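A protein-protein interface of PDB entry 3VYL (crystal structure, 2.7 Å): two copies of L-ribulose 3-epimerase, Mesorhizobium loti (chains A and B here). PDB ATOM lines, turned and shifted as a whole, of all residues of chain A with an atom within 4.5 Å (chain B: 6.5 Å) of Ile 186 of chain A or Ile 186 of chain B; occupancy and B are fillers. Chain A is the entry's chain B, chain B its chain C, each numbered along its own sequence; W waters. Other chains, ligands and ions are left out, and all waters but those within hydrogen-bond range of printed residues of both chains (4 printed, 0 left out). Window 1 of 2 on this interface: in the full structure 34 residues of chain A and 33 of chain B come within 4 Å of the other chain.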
ATOM      1  N   ASN A 150      14.528   1.351 -25.974  1.00  0.00           N
ATOM      2  CA  ASN A 150      14.118   0.037 -26.399  1.00  0.00           C
ATOM      3  C   ASN A 150      13.661   0.012 -27.860  1.00  0.00           C
ATOM      4  O   ASN A 150      13.392   1.058 -28.464  1.00  0.00           O
ATOM      5  CB  ASN A 150      13.043  -0.498 -25.459  1.00  0.00           C
ATOM      6  CG  ASN A 150      11.711   0.178 -25.662  1.00  0.00           C
ATOM      7  OD1 ASN A 150      11.052  -0.013 -26.681  1.00  0.00           O
ATOM      8  ND2 ASN A 150      11.307   0.979 -24.692  1.00  0.00           N
ATOM      9  N   PHE A 182      15.015   1.463 -17.472  1.00  0.00           N
ATOM     10  CA  PHE A 182      13.847   0.839 -18.103  1.00  0.00           C
ATOM     11  C   PHE A 182      14.156   0.300 -19.517  1.00  0.00           C
ATOM     12  O   PHE A 182      13.706  -0.790 -19.880  1.00  0.00           O
ATOM     13  CB  PHE A 182      12.663   1.807 -18.139  1.00  0.00           C
ATOM     14  CG  PHE A 182      11.630   1.461 -19.161  1.00  0.00           C
ATOM     15  CD1 PHE A 182      10.585   0.597 -18.847  1.00  0.00           C
ATOM     16  CD2 PHE A 182      11.695   2.003 -20.441  1.00  0.00           C
ATOM     17  CE1 PHE A 182       9.621   0.289 -19.791  1.00  0.00           C
ATOM     18  CE2 PHE A 182      10.742   1.690 -21.391  1.00  0.00           C
ATOM     19  CZ  PHE A 182       9.702   0.830 -21.064  1.00  0.00           C
ATOM     20  N   HIS A 183      14.913   1.058 -20.304  1.00  0.00           N
ATOM     21  CA  HIS A 183      15.267   0.596 -21.640  1.00  0.00           C
ATOM     22  C   HIS A 183      16.303  -0.492 -21.576  1.00  0.00           C
ATOM     23  O   HIS A 183      16.104  -1.577 -22.142  1.00  0.00           O
ATOM     24  CB  HIS A 183      15.716   1.750 -22.520  1.00  0.00           C
ATOM     25  CG  HIS A 183      14.636   2.787 -22.759  1.00  0.00           C
ATOM     26  ND1 HIS A 183      13.459   2.491 -23.365  1.00  0.00           N
ATOM     27  CD2 HIS A 183      14.587   4.139 -22.453  1.00  0.00           C
ATOM     28  CE1 HIS A 183      12.705   3.599 -23.434  1.00  0.00           C
ATOM     29  NE2 HIS A 183      13.395   4.605 -22.877  1.00  0.00           N
ATOM     30  N   MET A 184      17.390  -0.210 -20.857  1.00  0.00           N
ATOM     31  CA  MET A 184      18.488  -1.142 -20.628  1.00  0.00           C
ATOM     32  C   MET A 184      18.037  -2.530 -20.213  1.00  0.00           C
ATOM     33  O   MET A 184      18.556  -3.520 -20.724  1.00  0.00           O
ATOM     34  CB  MET A 184      19.468  -0.600 -19.576  1.00  0.00           C
ATOM     35  CG  MET A 184      20.418   0.454 -20.098  1.00  0.00           C
ATOM     36  SD  MET A 184      21.858   0.704 -19.053  1.00  0.00           S
ATOM     37  CE  MET A 184      21.105   1.277 -17.531  1.00  0.00           C
ATOM     38  N   ASN A 185      17.085  -2.611 -19.292  1.00  0.00           N
ATOM     39  CA  ASN A 185      16.602  -3.911 -18.838  1.00  0.00           C
ATOM     40  C   ASN A 185      15.923  -4.725 -19.953  1.00  0.00           C
ATOM     41  O   ASN A 185      15.861  -5.957 -19.873  1.00  0.00           O
ATOM     42  CB  ASN A 185      15.679  -3.765 -17.621  1.00  0.00           C
ATOM     43  CG  ASN A 185      15.490  -5.074 -16.857  1.00  0.00           C
ATOM     44  OD1 ASN A 185      16.432  -5.620 -16.274  1.00  0.00           O
ATOM     45  ND2 ASN A 185      14.263  -5.566 -16.836  1.00  0.00           N
ATOM     46  N   ILE A 186      15.406  -4.044 -20.981  1.00  0.00           N
ATOM     47  CA  ILE A 186      14.844  -4.748 -22.138  1.00  0.00           C
ATOM     48  C   ILE A 186      15.948  -5.173 -23.121  1.00  0.00           C
ATOM     49  O   ILE A 186      16.032  -6.353 -23.473  1.00  0.00           O
ATOM     50  CB  ILE A 186      13.748  -3.937 -22.866  1.00  0.00           C
ATOM     51  CG1 ILE A 186      12.505  -3.770 -21.988  1.00  0.00           C
ATOM     52  CG2 ILE A 186      13.335  -4.638 -24.145  1.00  0.00           C
ATOM     53  CD1 ILE A 186      11.694  -2.518 -22.288  1.00  0.00           C
ATOM     54  N   GLU A 187      16.809  -4.237 -23.525  1.00  0.00           N
ATOM     55  CA  GLU A 187      17.775  -4.489 -24.602  1.00  0.00           C
ATOM     56  C   GLU A 187      19.164  -5.027 -24.198  1.00  0.00           C
ATOM     57  O   GLU A 187      19.760  -5.808 -24.940  1.00  0.00           O
ATOM     58  CB  GLU A 187      17.984  -3.222 -25.454  1.00  0.00           C
ATOM     59  CG  GLU A 187      16.746  -2.599 -26.074  1.00  0.00           C
ATOM     60  CD  GLU A 187      15.992  -3.542 -26.988  1.00  0.00           C
ATOM     61  OE1 GLU A 187      16.619  -4.388 -27.673  1.00  0.00           O
ATOM     62  OE2 GLU A 187      14.751  -3.436 -27.020  1.00  0.00           O
ATOM     63  N   GLU A 188      19.698  -4.583 -23.060  1.00  0.00           N
ATOM     64  CA  GLU A 188      21.070  -4.933 -22.669  1.00  0.00           C
ATOM     65  C   GLU A 188      21.184  -6.387 -22.235  1.00  0.00           C
ATOM     66  O   GLU A 188      20.257  -6.940 -21.630  1.00  0.00           O
ATOM     67  CB  GLU A 188      21.578  -4.035 -21.540  1.00  0.00           C
ATOM     68  CG  GLU A 188      21.630  -2.552 -21.851  1.00  0.00           C
ATOM     69  CD  GLU A 188      22.676  -2.185 -22.883  1.00  0.00           C
ATOM     70  OE1 GLU A 188      23.583  -2.998 -23.141  1.00  0.00           O
ATOM     71  OE2 GLU A 188      22.598  -1.069 -23.438  1.00  0.00           O
ATOM     72  N   SER A 210      10.996  -1.501 -14.375  1.00  0.00           N
ATOM     73  CA  SER A 210      10.663  -2.317 -15.534  1.00  0.00           C
ATOM     74  C   SER A 210       9.284  -2.002 -16.097  1.00  0.00           C
ATOM     75  O   SER A 210       9.086  -2.083 -17.301  1.00  0.00           O
ATOM     76  CB  SER A 210      10.774  -3.808 -15.188  1.00  0.00           C
ATOM     77  OG  SER A 210       9.975  -4.164 -14.065  1.00  0.00           O
ATOM     78  N   HIS A 211       8.342  -1.633 -15.232  1.00  0.00           N
ATOM     79  CA  HIS A 211       6.982  -1.297 -15.667  1.00  0.00           C
ATOM     80  C   HIS A 211       6.695   0.185 -15.650  1.00  0.00           C
ATOM     81  O   HIS A 211       5.600   0.610 -16.015  1.00  0.00           O
ATOM     82  CB  HIS A 211       5.956  -2.040 -14.823  1.00  0.00           C
ATOM     83  CG  HIS A 211       6.174  -1.907 -13.327  1.00  0.00           C
ATOM     84  ND1 HIS A 211       6.599  -0.755 -12.744  1.00  0.00           N
ATOM     85  CD2 HIS A 211       5.982  -2.830 -12.290  1.00  0.00           C
ATOM     86  CE1 HIS A 211       6.668  -0.935 -11.415  1.00  0.00           C
ATOM     87  NE2 HIS A 211       6.295  -2.211 -11.140  1.00  0.00           N
ATOM     88  N   ASN B 150       3.349  -7.158 -23.790  1.00  0.00           N
ATOM     89  CA  ASN B 150       3.719  -5.856 -23.301  1.00  0.00           C
ATOM     90  C   ASN B 150       2.901  -4.749 -23.977  1.00  0.00           C
ATOM     91  O   ASN B 150       2.301  -4.972 -25.036  1.00  0.00           O
ATOM     92  CB  ASN B 150       5.211  -5.630 -23.521  1.00  0.00           C
ATOM     93  CG  ASN B 150       5.575  -5.648 -24.977  1.00  0.00           C
ATOM     94  OD1 ASN B 150       5.971  -6.685 -25.514  1.00  0.00           O
ATOM     95  ND2 ASN B 150       5.398  -4.518 -25.641  1.00  0.00           N
ATOM     96  N   ARG B 151       2.916  -3.564 -23.352  1.00  0.00           N
ATOM     97  CA  ARG B 151       2.187  -2.359 -23.781  1.00  0.00           C
ATOM     98  C   ARG B 151       2.304  -1.974 -25.276  1.00  0.00           C
ATOM     99  O   ARG B 151       1.368  -1.408 -25.851  1.00  0.00           O
ATOM    100  CB  ARG B 151       2.623  -1.177 -22.921  1.00  0.00           C
ATOM    101  CG  ARG B 151       4.107  -0.828 -23.067  1.00  0.00           C
ATOM    102  CD  ARG B 151       4.674  -0.063 -21.881  1.00  0.00           C
ATOM    103  NE  ARG B 151       4.418  -0.728 -20.602  1.00  0.00           N
ATOM    104  CZ  ARG B 151       4.670  -0.178 -19.411  1.00  0.00           C
ATOM    105  NH1 ARG B 151       5.212   1.043 -19.341  1.00  0.00           N
ATOM    106  NH2 ARG B 151       4.383  -0.848 -18.290  1.00  0.00           N
ATOM    107  N   PHE B 152       3.443  -2.268 -25.898  1.00  0.00           N
ATOM    108  CA  PHE B 152       3.636  -1.946 -27.310  1.00  0.00           C
ATOM    109  C   PHE B 152       3.066  -2.986 -28.276  1.00  0.00           C
ATOM    110  O   PHE B 152       3.130  -2.796 -29.482  1.00  0.00           O
ATOM    111  CB  PHE B 152       5.110  -1.757 -27.613  1.00  0.00           C
ATOM    112  CG  PHE B 152       5.797  -0.752 -26.733  1.00  0.00           C
ATOM    113  CD1 PHE B 152       5.708   0.613 -27.007  1.00  0.00           C
ATOM    114  CD2 PHE B 152       6.564  -1.170 -25.657  1.00  0.00           C
ATOM    115  CE1 PHE B 152       6.358   1.540 -26.205  1.00  0.00           C
ATOM    116  CE2 PHE B 152       7.213  -0.242 -24.843  1.00  0.00           C
ATOM    117  CZ  PHE B 152       7.115   1.112 -25.121  1.00  0.00           C
ATOM    118  N   THR B 181       7.466 -14.906 -20.571  1.00  0.00           N
ATOM    119  CA  THR B 181       8.453 -14.286 -19.671  1.00  0.00           C
ATOM    120  C   THR B 181       9.053 -12.974 -20.198  1.00  0.00           C
ATOM    121  O   THR B 181       9.333 -12.085 -19.405  1.00  0.00           O
ATOM    122  CB  THR B 181       9.585 -15.238 -19.242  1.00  0.00           C
ATOM    123  OG1 THR B 181      10.374 -15.596 -20.380  1.00  0.00           O
ATOM    124  CG2 THR B 181       9.034 -16.501 -18.575  1.00  0.00           C
ATOM    125  N   PHE B 182       9.235 -12.855 -21.519  1.00  0.00           N
ATOM    126  CA  PHE B 182       9.672 -11.600 -22.152  1.00  0.00           C
ATOM    127  C   PHE B 182       8.729 -10.428 -21.829  1.00  0.00           C
ATOM    128  O   PHE B 182       9.179  -9.327 -21.458  1.00  0.00           O
ATOM    129  CB  PHE B 182       9.817 -11.756 -23.683  1.00  0.00           C
ATOM    130  CG  PHE B 182       9.939 -10.441 -24.432  1.00  0.00           C
ATOM    131  CD1 PHE B 182      11.133  -9.731 -24.446  1.00  0.00           C
ATOM    132  CD2 PHE B 182       8.855  -9.914 -25.126  1.00  0.00           C
ATOM    133  CE1 PHE B 182      11.237  -8.511 -25.122  1.00  0.00           C
ATOM    134  CE2 PHE B 182       8.959  -8.701 -25.810  1.00  0.00           C
ATOM    135  CZ  PHE B 182      10.152  -7.994 -25.805  1.00  0.00           C
ATOM    136  N   HIS B 183       7.429 -10.666 -21.994  1.00  0.00           N
ATOM    137  CA  HIS B 183       6.436  -9.644 -21.742  1.00  0.00           C
ATOM    138  C   HIS B 183       6.270  -9.439 -20.259  1.00  0.00           C
ATOM    139  O   HIS B 183       6.200  -8.305 -19.789  1.00  0.00           O
ATOM    140  CB  HIS B 183       5.112 -10.010 -22.397  1.00  0.00           C
ATOM    141  CG  HIS B 183       5.185 -10.140 -23.908  1.00  0.00           C
ATOM    142  ND1 HIS B 183       5.598  -9.131 -24.716  1.00  0.00           N
ATOM    143  CD2 HIS B 183       4.850 -11.204 -24.748  1.00  0.00           C
ATOM    144  CE1 HIS B 183       5.547  -9.536 -26.001  1.00  0.00           C
ATOM    145  NE2 HIS B 183       5.092 -10.806 -26.021  1.00  0.00           N
ATOM    146  N   MET B 184       6.224 -10.539 -19.510  1.00  0.00           N
ATOM    147  CA  MET B 184       6.061 -10.476 -18.063  1.00  0.00           C
ATOM    148  C   MET B 184       7.140  -9.610 -17.424  1.00  0.00           C
ATOM    149  O   MET B 184       6.843  -8.837 -16.512  1.00  0.00           O
ATOM    150  CB  MET B 184       6.037 -11.869 -17.425  1.00  0.00           C
ATOM    151  CG  MET B 184       4.743 -12.598 -17.697  1.00  0.00           C
ATOM    152  SD  MET B 184       4.407 -14.015 -16.648  1.00  0.00           S
ATOM    153  CE  MET B 184       5.620 -15.182 -17.255  1.00  0.00           C
ATOM    154  N   ASN B 185       8.377  -9.712 -17.914  1.00  0.00           N
ATOM    155  CA  ASN B 185       9.473  -8.950 -17.336  1.00  0.00           C
ATOM    156  C   ASN B 185       9.297  -7.446 -17.505  1.00  0.00           C
ATOM    157  O   ASN B 185       9.737  -6.675 -16.665  1.00  0.00           O
ATOM    158  CB  ASN B 185      10.829  -9.381 -17.893  1.00  0.00           C
ATOM    159  CG  ASN B 185      11.945  -9.229 -16.874  1.00  0.00           C
ATOM    160  OD1 ASN B 185      11.852  -9.742 -15.740  1.00  0.00           O
ATOM    161  ND2 ASN B 185      13.004  -8.529 -17.262  1.00  0.00           N
ATOM    162  N   ILE B 186       8.654  -7.039 -18.593  1.00  0.00           N
ATOM    163  CA  ILE B 186       8.309  -5.643 -18.814  1.00  0.00           C
ATOM    164  C   ILE B 186       7.070  -5.235 -18.019  1.00  0.00           C
ATOM    165  O   ILE B 186       7.027  -4.125 -17.495  1.00  0.00           O
ATOM    166  CB  ILE B 186       8.023  -5.348 -20.296  1.00  0.00           C
ATOM    167  CG1 ILE B 186       9.255  -5.620 -21.152  1.00  0.00           C
ATOM    168  CG2 ILE B 186       7.545  -3.906 -20.463  1.00  0.00           C
ATOM    169  CD1 ILE B 186       8.930  -5.864 -22.614  1.00  0.00           C
ATOM    170  N   GLU B 187       6.068  -6.115 -17.932  1.00  0.00           N
ATOM    171  CA  GLU B 187       4.739  -5.689 -17.460  1.00  0.00           C
ATOM    172  C   GLU B 187       4.448  -6.045 -16.014  1.00  0.00           C
ATOM    173  O   GLU B 187       3.908  -5.232 -15.268  1.00  0.00           O
ATOM    174  CB  GLU B 187       3.608  -6.202 -18.377  1.00  0.00           C
ATOM    175  CG  GLU B 187       3.605  -5.660 -19.802  1.00  0.00           C
ATOM    176  CD  GLU B 187       3.541  -4.145 -19.878  1.00  0.00           C
ATOM    177  OE1 GLU B 187       2.909  -3.516 -19.000  1.00  0.00           O
ATOM    178  OE2 GLU B 187       4.124  -3.568 -20.820  1.00  0.00           O
ATOM    179  N   GLU B 188       4.798  -7.265 -15.624  1.00  0.00           N
ATOM    180  CA  GLU B 188       4.525  -7.741 -14.271  1.00  0.00           C
ATOM    181  C   GLU B 188       5.365  -7.051 -13.191  1.00  0.00           C
ATOM    182  O   GLU B 188       6.463  -6.562 -13.450  1.00  0.00           O
ATOM    183  CB  GLU B 188       4.698  -9.255 -14.192  1.00  0.00           C
ATOM    184  CG  GLU B 188       3.898 -10.021 -15.236  1.00  0.00           C
ATOM    185  CD  GLU B 188       2.397  -9.951 -15.025  1.00  0.00           C
ATOM    186  OE1 GLU B 188       1.938  -9.624 -13.902  1.00  0.00           O
ATOM    187  OE2 GLU B 188       1.668 -10.239 -15.998  1.00  0.00           O
ATOM    188  N   VAL B 191       7.673 -11.573 -11.740  1.00  0.00           N
ATOM    189  CA  VAL B 191       7.295 -12.640 -12.646  1.00  0.00           C
ATOM    190  C   VAL B 191       6.809 -13.874 -11.887  1.00  0.00           C
ATOM    191  O   VAL B 191       5.781 -14.442 -12.240  1.00  0.00           O
ATOM    192  CB  VAL B 191       8.407 -12.969 -13.655  1.00  0.00           C
ATOM    193  CG1 VAL B 191       7.951 -14.078 -14.592  1.00  0.00           C
ATOM    194  CG2 VAL B 191       8.746 -11.731 -14.455  1.00  0.00           C
ATOM    195  N   GLU B 209      13.976 -14.592 -23.286  1.00  0.00           N
ATOM    196  CA  GLU B 209      14.863 -13.742 -22.520  1.00  0.00           C
ATOM    197  C   GLU B 209      14.482 -12.274 -22.729  1.00  0.00           C
ATOM    198  O   GLU B 209      13.815 -11.936 -23.704  1.00  0.00           O
ATOM    199  CB  GLU B 209      16.308 -14.025 -22.949  1.00  0.00           C
ATOM    200  CG  GLU B 209      17.391 -13.181 -22.296  1.00  0.00           C
ATOM    201  CD  GLU B 209      17.519 -13.416 -20.802  1.00  0.00           C
ATOM    202  OE1 GLU B 209      18.385 -14.221 -20.410  1.00  0.00           O
ATOM    203  OE2 GLU B 209      16.771 -12.800 -20.015  1.00  0.00           O
ATOM    204  N   SER B 210      14.899 -11.422 -21.793  1.00  0.00           N
ATOM    205  CA  SER B 210      14.660  -9.988 -21.807  1.00  0.00           C
ATOM    206  C   SER B 210      14.821  -9.344 -23.180  1.00  0.00           C
ATOM    207  O   SER B 210      14.000  -8.514 -23.566  1.00  0.00           O
ATOM    208  CB  SER B 210      15.573  -9.293 -20.775  1.00  0.00           C
ATOM    209  OG  SER B 210      16.958  -9.289 -21.160  1.00  0.00           O
ATOM    210  N   HIS B 211      15.876  -9.721 -23.910  1.00  0.00           N
ATOM    211  CA  HIS B 211      16.141  -9.169 -25.259  1.00  0.00           C
ATOM    212  C   HIS B 211      15.710 -10.100 -26.368  1.00  0.00           C
ATOM    213  O   HIS B 211      15.848  -9.769 -27.550  1.00  0.00           O
ATOM    214  CB  HIS B 211      17.614  -8.815 -25.429  1.00  0.00           C
ATOM    215  CG  HIS B 211      18.553  -9.936 -25.049  1.00  0.00           C
ATOM    216  ND1 HIS B 211      18.346 -11.217 -25.422  1.00  0.00           N
ATOM    217  CD2 HIS B 211      19.726  -9.931 -24.311  1.00  0.00           C
ATOM    218  CE1 HIS B 211      19.325 -11.991 -24.936  1.00  0.00           C
ATOM    219  NE2 HIS B 211      20.169 -11.205 -24.252  1.00  0.00           N
ATOM    220  N   ARG B 212      15.203 -11.277 -25.996  1.00  0.00           N
ATOM    221  CA  ARG B 212      14.676 -12.255 -26.958  1.00  0.00           C
ATOM    222  C   ARG B 212      15.738 -13.098 -27.675  1.00  0.00           C
ATOM    223  O   ARG B 212      15.419 -13.778 -28.641  1.00  0.00           O
ATOM    224  CB  ARG B 212      13.761 -11.564 -27.983  1.00  0.00           C
ATOM    225  CG  ARG B 212      12.288 -11.946 -27.894  1.00  0.00           C
ATOM    226  CD  ARG B 212      11.427 -10.711 -27.705  1.00  0.00           C
ATOM    227  NE  ARG B 212      10.062 -10.794 -28.245  1.00  0.00           N
ATOM    228  CZ  ARG B 212       9.163 -11.749 -27.997  1.00  0.00           C
ATOM    229  NH1 ARG B 212       9.435 -12.790 -27.234  1.00  0.00           N
ATOM    230  NH2 ARG B 212       7.972 -11.664 -28.551  1.00  0.00           N
ATOM    231  N   ASN B 219      18.486 -10.174 -18.808  1.00  0.00           N
ATOM    232  CA  ASN B 219      18.212  -9.715 -17.451  1.00  0.00           C
ATOM    233  C   ASN B 219      17.158 -10.511 -16.656  1.00  0.00           C
ATOM    234  O   ASN B 219      16.812 -10.138 -15.527  1.00  0.00           O
ATOM    235  CB  ASN B 219      17.799  -8.241 -17.514  1.00  0.00           C
ATOM    236  CG  ASN B 219      18.879  -7.358 -18.121  1.00  0.00           C
ATOM    237  OD1 ASN B 219      20.006  -7.301 -17.611  1.00  0.00           O
ATOM    238  ND2 ASN B 219      18.552  -6.670 -19.209  1.00  0.00           N
ATOM    239  N   ARG B 260      18.047  -6.487 -34.565  1.00  0.00           N
ATOM    240  CA  ARG B 260      19.407  -6.889 -34.220  1.00  0.00           C
ATOM    241  C   ARG B 260      19.717  -8.364 -34.390  1.00  0.00           C
ATOM    242  O   ARG B 260      18.861  -9.228 -34.218  1.00  0.00           O
ATOM    243  CB  ARG B 260      19.753  -6.448 -32.802  1.00  0.00           C
ATOM    244  CG  ARG B 260      19.798  -4.942 -32.610  1.00  0.00           C
ATOM    245  CD  ARG B 260      20.394  -4.581 -31.262  1.00  0.00           C
ATOM    246  NE  ARG B 260      19.508  -4.965 -30.174  1.00  0.00           N
ATOM    247  CZ  ARG B 260      19.917  -5.457 -29.006  1.00  0.00           C
ATOM    248  NH1 ARG B 260      21.216  -5.645 -28.778  1.00  0.00           N
ATOM    249  NH2 ARG B 260      19.020  -5.777 -28.074  1.00  0.00           N
HETATM  250  O   HOH W   1      14.979  -8.204 -14.825  1.00  0.00           O
HETATM  251  O   HOH W   2      12.037  -4.847 -17.893  1.00  0.00           O
HETATM  252  O   HOH W   3      13.086  -7.007 -19.433  1.00  0.00           O
HETATM  253  O   HOH W   4      17.173  -3.817 -30.283  1.00  0.00           O
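The backbone NH (N) of His 211 of chain B lies close to the backbone carbonyl oxygen (O) of Ile 186 of chain A, at 3.4 Å. The backbone carbonyl oxygen of Ile 186 of chain B sits close to the backbone carbonyl oxygen of Ser 210 of chain A (2.9 Å). The backbone carbonyl oxygen (O) of Asn 185 of chain A lies within hydrogen-bond range of the side-chain amide nitrogen (ND2) of Asn 219 of chain B (2.9 Å). The side-chain amide nitrogen (ND2) of Asn 185 of chain A sits close to the side-chain amide nitrogen (ND2) of Asn 185 of chain B, 3.2 Å away. The side-chain carboxylate (OE1) of Glu 187 of chain A lies within salt-bridge range of the guanidinium group (NH2) of Arg 260 of chain B. The backbone carbonyl oxygen (O) of Ser 210 of chain B sits close to the backbone carbonyl oxygen (O) of Ile 186 of chain A, 3.0 Å away. The backbone carbonyl oxygen of Met 184 of chain A lies within hydrogen-bond range of the side-chain amide nitrogen of Asn 219 of chain B (3.5 Å). The side-chain amide nitrogen (ND2) of Asn 219 of chain B is in hydrogen-bond range of the backbone carbonyl oxygen (O) of Glu 188 of chain A, 3.0 Å away. The backbone carbonyl oxygen of His 211 of chain A is in hydrogen-bond range of the guanidinium group of Arg 151 of chain B, 3.0 Å away.
Water W2 bridges the side-chain amide nitrogen of Asn 185 of chain A (2.6 Å) and the backbone carbonyl oxygen of Asn 185 of chain B (3.2 Å). Water W4 bridges the guanidinium group of Arg 260 of chain B (2.6 Å) and the side-chain carboxylate of Glu 187 of chain A (2.7 Å). Water W3 bridges ND2 of Asn 185 of chain B and O of Asn 185 of chain A. Water W1 lies within hydrogen-bond range of O of Asn 219 of chain B (2.8 Å), ND2 of Asn 185 of chain B (3.2 Å) and OD1 of Asn 185 of chain A (3.3 Å).
Asn 185 of chain A touches Ser 210 of chain B (O to CB, 3.5 Å). CG1 of Ile 186 of chain A touches CG1 of Ile 186 of chain B, at 3.8 Å. Glu 187 of chain A touches His 211 of chain B. Asn 185 of chain B touches Ser 210 of chain A (O to CB, 3.4 Å). Ile 186 of chain B touches His 211 of chain A (O to CA, 3.4 Å). CB of His 211 of chain A touches O of Glu 187 of chain B (3.8 Å). His 211 of chain A touches Glu 188 of chain B (CD2 to O, 3.9 Å).
Ile 186 of chain A touches just these residues of chain B: Ile 186, Ser 210 and His 211. Ile 186 of chain B touches just these residues of chain A: Ile 186 (3.8 Å), Ser 210 (2.9 Å) and His 211 (3.4 Å). Printed residues of chain B within 4 Å of Met 184 of chain A: Asn 219. Printed residues of chain A within 4 Å of Ser 210 of chain B: Asn 185 and Ile 186. Printed residues of chain A within 4 Å of Arg 151 of chain B: His 211 (3.0 Å). Phe 182 of chain B touches none of the printed residues of chain A. Asn 150 of chain B touches none of the printed residues of chain A. The nearest residue of chain B that does not touch Ile 186 of chain A is Asn 219 of chain B (4.5 Å). The nearest printed residue of chain A that does not touch Ile 186 of chain B is Phe 182 of chain A (4.7 Å).
The backbone NH of Asn 219 of chain B is in hydrogen-bond range of the side-chain carboxylate of Glu 209 of chain B (3.4 Å). NE of Arg 151 of chain B lies within salt-bridge range of OE2 of Glu 187 of chain B (2.9 Å). The side-chain hydroxyl (OG) of Ser 210 of chain B sits at hydrogen-bond distance from the backbone NH (N) of Asn 219 of chain B (2.9 Å).
Of the 18 printed residues of chain B, 9 touch a printed residue of chain A. Hydrophobic or aromatic side chains of chain B within 4 Å of the printed part of chain A: Ile 186 and His 211. Of the 10 printed residues of chain A, 7 touch a printed residue of chain B. Printed residues of chain A that touch a printed residue of chain B: Met 184, Asn 185, Ile 186, Glu 187, Glu 188, Ser 210 and His 211. Among the printed residues, Asp or Glu carboxylates within 4 Å of a Lys or Arg side-chain nitrogen of the other chain: Glu 187 of chain A with Arg 260 of chain B (2.8 Å).
Asn 185 of chain A touches Ser 210 of chain B, and with the chains exchanged Ser 210 of chain A touches Asn 185 of chain B. Ile 186 of chain B touches its own counterpart, Ile 186 of chain A. Glu 187 of chain A touches His 211 of chain B, and with the chains exchanged His 211 of chain A touches Glu 187 of chain B. His 211 of chain A touches Glu 188 of chain B, but with the chains exchanged Glu 188 of chain A does not touch His 211 of chain B (4.1 Å). 10 positions are printed for both chains. Of the 16 pairs that touch across the chains among the printed residues, 10 have their exchanged pair printed and touching as well.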
